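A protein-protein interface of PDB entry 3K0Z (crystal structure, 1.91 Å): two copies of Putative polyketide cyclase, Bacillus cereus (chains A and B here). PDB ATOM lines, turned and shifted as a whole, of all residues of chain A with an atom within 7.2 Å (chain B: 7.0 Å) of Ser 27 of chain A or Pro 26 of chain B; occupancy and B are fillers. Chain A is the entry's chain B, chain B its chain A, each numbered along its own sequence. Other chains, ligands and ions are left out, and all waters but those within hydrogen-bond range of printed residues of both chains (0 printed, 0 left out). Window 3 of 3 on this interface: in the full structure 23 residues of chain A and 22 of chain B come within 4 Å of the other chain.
OD1 of Asp 25 of chain B lies close to OD1 of Asp 25 of chain A, 3.5 Å away.
Hydrophobic or aromatic side chains of chain A within 4 Å of the printed part of chain B: Pro 26 and Val 103. Of the 8 printed residues of chain B, 5 touch a printed residue of chain A. Printed residues of chain B that touch a printed residue of chain A: Thr 23, Asp 25, Pro 26, Ser 27 and Val 102. Among the printed residues, no Asp or Glu carboxylate lies within 4 Å of a Lys or Arg side-chain nitrogen of the other chain.
Printed residues of chain B within 4 Å of Ser 27 of chain A: Pro 26 (3.5 Å). Pro 26 of chain B touches two residues of chain A. Of the printed residues of chain A, Ser 27 of chain B touches Pro 26. Printed residues of chain B within 4 Å of Asp 25 of chain A: Asp 25 and Pro 26. Of the printed residues of chain B, Val 103 of chain A touches Thr 23, Asp 25 and Val 102. The nearest printed residue of chain B that does not touch Ser 27 of chain A is Asp 25 of chain B (5.2 Å). The nearest printed residue of chain A that does not touch Val 102 of chain B is Asp 25 of chain A (6.8 Å).
OD1 of Asp 25 of chain A touches CD of Pro 26 of chain B (3.6 Å). Pro 26 of chain A touches Asp 25 of chain B (CD to OD1, 3.6 Å). Pro 26 of chain A touches Ser 27 of chain B. Ser 27 of chain A touches Pro 26 of chain B (OG to CG, 3.5 Å). Val 103 of chain A touches Thr 23 of chain B. Val 103 of chain A touches Asp 25 of chain B. Val 102 of chain B touches Val 103 of chain A (O to CG2, 3.7 Å).
The side-chain carboxylate (OD1) of Asp 25 of chain B sits at hydrogen-bond distance from the side-chain hydroxyl (OG) of Ser 27 of chain B (2.5 Å). N of Gly 104 of chain A lies within hydrogen-bond range of OD2 of Asp 25 of chain A (3.1 Å). N of Val 102 of chain B lies within hydrogen-bond range of O of Thr 23 of chain B, 2.7 Å away. The backbone NH of Asp 25 of chain B lies within hydrogen-bond range of the backbone carbonyl oxygen of Val 102 of chain B (2.9 Å). The side-chain hydroxyl of Ser 27 of chain A is in hydrogen-bond range of the side-chain carboxylate of Asp 25 of chain A (2.8 Å).
Asp 25 of chain B touches its own counterpart, Asp 25 of chain A. Asp 25 of chain A touches Pro 26 of chain B, and with the chains exchanged Pro 26 of chain A touches Asp 25 of chain B. Pro 26 of chain A touches Ser 27 of chain B, and with the chains exchanged Ser 27 of chain A touches Pro 26 of chain B. 6 positions are printed for both chains. Of the 8 pairs that touch across the chains among the printed residues, 5 have their exchanged pair printed and touching as well.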
ATOM      1  N   ILE A  24       8.772  24.520 -23.248  1.00  0.00           N
ATOM      2  CA  ILE A  24       8.498  25.754 -23.924  1.00  0.00           C
ATOM      3  C   ILE A  24       7.232  25.686 -24.758  1.00  0.00           C
ATOM      4  O   ILE A  24       7.019  24.732 -25.508  1.00  0.00           O
ATOM      5  CB  ILE A  24       9.658  26.110 -24.862  1.00  0.00           C
ATOM      6  CG1 ILE A  24      10.966  26.350 -24.075  1.00  0.00           C
ATOM      7  CG2 ILE A  24       9.327  27.336 -25.638  1.00  0.00           C
ATOM      8  CD1 ILE A  24      12.155  26.311 -24.997  1.00  0.00           C
ATOM      9  N   ASP A  25       6.397  26.713 -24.609  1.00  0.00           N
ATOM     10  CA  ASP A  25       5.181  26.897 -25.387  1.00  0.00           C
ATOM     11  C   ASP A  25       5.577  26.894 -26.872  1.00  0.00           C
ATOM     12  O   ASP A  25       6.311  27.768 -27.316  1.00  0.00           O
ATOM     13  CB  ASP A  25       4.591  28.234 -24.932  1.00  0.00           C
ATOM     14  CG  ASP A  25       3.384  28.688 -25.689  1.00  0.00           C
ATOM     15  OD1 ASP A  25       2.959  28.062 -26.692  1.00  0.00           O
ATOM     16  OD2 ASP A  25       2.825  29.715 -25.203  1.00  0.00           O
ATOM     17  N   PRO A  26       5.123  25.896 -27.632  1.00  0.00           N
ATOM     18  CA  PRO A  26       5.539  25.838 -29.032  1.00  0.00           C
ATOM     19  C   PRO A  26       4.856  26.799 -29.982  1.00  0.00           C
ATOM     20  O   PRO A  26       5.231  26.842 -31.136  1.00  0.00           O
ATOM     21  CB  PRO A  26       5.207  24.396 -29.435  1.00  0.00           C
ATOM     22  CG  PRO A  26       4.137  23.980 -28.551  1.00  0.00           C
ATOM     23  CD  PRO A  26       4.302  24.729 -27.260  1.00  0.00           C
ATOM     24  N   SER A  27       3.917  27.605 -29.518  1.00  0.00           N
ATOM     25  CA  SER A  27       3.274  28.594 -30.378  1.00  0.00           C
ATOM     26  C   SER A  27       4.120  29.864 -30.471  1.00  0.00           C
ATOM     27  O   SER A  27       3.916  30.702 -31.338  1.00  0.00           O
ATOM     28  CB  SER A  27       1.902  28.926 -29.821  1.00  0.00           C
ATOM     29  OG  SER A  27       1.988  29.747 -28.659  1.00  0.00           O
ATOM     30  N   LEU A  28       5.081  29.996 -29.578  1.00  0.00           N
ATOM     31  CA  LEU A  28       5.977  31.131 -29.566  1.00  0.00           C
ATOM     32  C   LEU A  28       6.932  31.040 -30.758  1.00  0.00           C
ATOM     33  O   LEU A  28       7.378  29.971 -31.126  1.00  0.00           O
ATOM     34  CB  LEU A  28       6.752  31.142 -28.251  1.00  0.00           C
ATOM     35  CG  LEU A  28       5.987  31.346 -26.941  1.00  0.00           C
ATOM     36  CD1 LEU A  28       6.929  31.182 -25.705  1.00  0.00           C
ATOM     37  CD2 LEU A  28       5.330  32.719 -26.937  1.00  0.00           C
ATOM     38  N   SER A  29       7.217  32.165 -31.381  1.00  0.00           N
ATOM     39  CA  SER A  29       8.149  32.195 -32.477  1.00  0.00           C
ATOM     40  C   SER A  29       9.531  31.897 -31.932  1.00  0.00           C
ATOM     41  O   SER A  29       9.763  31.971 -30.726  1.00  0.00           O
ATOM     42  CB  SER A  29       8.113  33.565 -33.154  1.00  0.00           C
ATOM     43  OG  SER A  29       8.793  34.544 -32.384  1.00  0.00           O
ATOM     44  N   GLN A  30      10.469  31.550 -32.815  1.00  0.00           N
ATOM     45  CA  GLN A  30      11.852  31.318 -32.359  1.00  0.00           C
ATOM     46  C   GLN A  30      12.418  32.559 -31.659  1.00  0.00           C
ATOM     47  O   GLN A  30      13.074  32.447 -30.636  1.00  0.00           O
ATOM     48  CB  GLN A  30      12.763  30.893 -33.557  1.00  0.00           C
ATOM     49  CG  GLN A  30      14.216  30.502 -33.221  1.00  0.00           C
ATOM     50  CD  GLN A  30      14.319  29.321 -32.278  1.00  0.00           C
ATOM     51  N   GLU A  32      10.750  35.013 -30.037  1.00  0.00           N
ATOM     52  CA  GLU A  32      10.015  35.169 -28.754  1.00  0.00           C
ATOM     53  C   GLU A  32      10.441  34.199 -27.708  1.00  0.00           C
ATOM     54  O   GLU A  32      10.660  34.561 -26.558  1.00  0.00           O
ATOM     55  CB  GLU A  32       8.518  34.952 -28.946  1.00  0.00           C
ATOM     56  CG  GLU A  32       7.808  35.999 -29.772  1.00  0.00           C
ATOM     57  CD  GLU A  32       6.313  35.662 -30.161  1.00  0.00           C
ATOM     58  OE1 GLU A  32       5.928  34.495 -30.483  1.00  0.00           O
ATOM     59  OE2 GLU A  32       5.528  36.628 -30.212  1.00  0.00           O
ATOM     60  N   VAL A 103       5.612  29.976 -21.069  1.00  0.00           N
ATOM     61  CA  VAL A 103       4.286  29.974 -21.676  1.00  0.00           C
ATOM     62  C   VAL A 103       3.695  31.374 -21.731  1.00  0.00           C
ATOM     63  O   VAL A 103       3.744  32.099 -20.773  1.00  0.00           O
ATOM     64  CB  VAL A 103       3.326  28.967 -20.960  1.00  0.00           C
ATOM     65  CG1 VAL A 103       3.109  29.291 -19.464  1.00  0.00           C
ATOM     66  CG2 VAL A 103       1.967  28.772 -21.734  1.00  0.00           C
ATOM     67  N   GLY A 104       3.157  31.749 -22.886  1.00  0.00           N
ATOM     68  CA  GLY A 104       2.611  33.084 -23.075  1.00  0.00           C
ATOM     69  C   GLY A 104       3.704  34.101 -22.736  1.00  0.00           C
ATOM     70  O   GLY A 104       4.792  34.058 -23.336  1.00  0.00           O
ATOM     71  N   THR B  23      -2.668  31.421 -17.653  1.00  0.00           N
ATOM     72  CA  THR B  23      -2.055  31.372 -18.942  1.00  0.00           C
ATOM     73  C   THR B  23      -1.995  29.900 -19.381  1.00  0.00           C
ATOM     74  O   THR B  23      -1.399  29.041 -18.708  1.00  0.00           O
ATOM     75  CB  THR B  23      -0.642  31.996 -18.895  1.00  0.00           C
ATOM     76  OG1 THR B  23      -0.752  33.359 -18.479  1.00  0.00           O
ATOM     77  CG2 THR B  23       0.025  31.913 -20.236  1.00  0.00           C
ATOM     78  N   ILE B  24      -2.629  29.608 -20.508  1.00  0.00           N
ATOM     79  CA  ILE B  24      -2.625  28.261 -21.052  1.00  0.00           C
ATOM     80  C   ILE B  24      -1.973  28.175 -22.437  1.00  0.00           C
ATOM     81  O   ILE B  24      -2.346  28.885 -23.371  1.00  0.00           O
ATOM     82  CB  ILE B  24      -4.029  27.681 -21.157  1.00  0.00           C
ATOM     83  CG1 ILE B  24      -4.797  27.857 -19.825  1.00  0.00           C
ATOM     84  CG2 ILE B  24      -3.893  26.218 -21.571  1.00  0.00           C
ATOM     85  CD1 ILE B  24      -6.311  27.485 -19.866  1.00  0.00           C
ATOM     86  N   ASP B  25      -1.008  27.271 -22.533  1.00  0.00           N
ATOM     87  CA  ASP B  25      -0.305  26.908 -23.784  1.00  0.00           C
ATOM     88  C   ASP B  25      -1.367  26.646 -24.868  1.00  0.00           C
ATOM     89  O   ASP B  25      -2.187  25.757 -24.708  1.00  0.00           O
ATOM     90  CB  ASP B  25       0.478  25.626 -23.447  1.00  0.00           C
ATOM     91  CG  ASP B  25       1.168  24.945 -24.624  1.00  0.00           C
ATOM     92  OD1 ASP B  25       1.007  25.315 -25.807  1.00  0.00           O
ATOM     93  OD2 ASP B  25       1.866  23.952 -24.306  1.00  0.00           O
ATOM     94  N   PRO B  26      -1.373  27.447 -25.944  1.00  0.00           N
ATOM     95  CA  PRO B  26      -2.341  27.322 -27.040  1.00  0.00           C
ATOM     96  C   PRO B  26      -2.321  26.013 -27.805  1.00  0.00           C
ATOM     97  O   PRO B  26      -3.289  25.681 -28.474  1.00  0.00           O
ATOM     98  CB  PRO B  26      -1.937  28.451 -27.998  1.00  0.00           C
ATOM     99  CG  PRO B  26      -1.146  29.373 -27.219  1.00  0.00           C
ATOM    100  CD  PRO B  26      -0.504  28.618 -26.122  1.00  0.00           C
ATOM    101  N   SER B  27      -1.234  25.271 -27.681  1.00  0.00           N
ATOM    102  CA  SER B  27      -1.052  24.039 -28.392  1.00  0.00           C
ATOM    103  C   SER B  27      -1.781  22.901 -27.710  1.00  0.00           C
ATOM    104  O   SER B  27      -2.034  21.901 -28.345  1.00  0.00           O
ATOM    105  CB  SER B  27       0.442  23.733 -28.519  1.00  0.00           C
ATOM    106  OG  SER B  27       0.961  23.249 -27.294  1.00  0.00           O
ATOM    107  N   LEU B  28      -2.152  23.050 -26.438  1.00  0.00           N
ATOM    108  CA  LEU B  28      -2.910  22.001 -25.743  1.00  0.00           C
ATOM    109  C   LEU B  28      -4.338  21.980 -26.304  1.00  0.00           C
ATOM    110  O   LEU B  28      -4.913  23.029 -26.545  1.00  0.00           O
ATOM    111  CB  LEU B  28      -2.920  22.258 -24.231  1.00  0.00           C
ATOM    112  CG  LEU B  28      -1.562  22.230 -23.514  1.00  0.00           C
ATOM    113  CD1 LEU B  28      -1.674  22.643 -22.053  1.00  0.00           C
ATOM    114  CD2 LEU B  28      -0.956  20.866 -23.617  1.00  0.00           C
ATOM    115  N   SER B  29      -4.894  20.791 -26.513  1.00  0.00           N
ATOM    116  CA  SER B  29      -6.288  20.661 -26.896  1.00  0.00           C
ATOM    117  C   SER B  29      -7.160  21.139 -25.740  1.00  0.00           C
ATOM    118  O   SER B  29      -6.732  21.176 -24.570  1.00  0.00           O
ATOM    119  CB  SER B  29      -6.640  19.199 -27.191  1.00  0.00           C
ATOM    120  OG  SER B  29      -6.795  18.511 -25.946  1.00  0.00           O
ATOM    121  N   VAL B 102      -0.164  26.953 -17.455  1.00  0.00           N
ATOM    122  CA  VAL B 102      -0.338  25.567 -17.955  1.00  0.00           C
ATOM    123  C   VAL B 102       0.433  25.341 -19.255  1.00  0.00           C
ATOM    124  O   VAL B 102       0.145  25.963 -20.242  1.00  0.00           O
ATOM    125  CB  VAL B 102      -1.829  25.230 -18.107  1.00  0.00           C
ATOM    126  CG1 VAL B 102      -1.993  23.792 -18.512  1.00  0.00           C
ATOM    127  CG2 VAL B 102      -2.621  25.554 -16.767  1.00  0.00           C
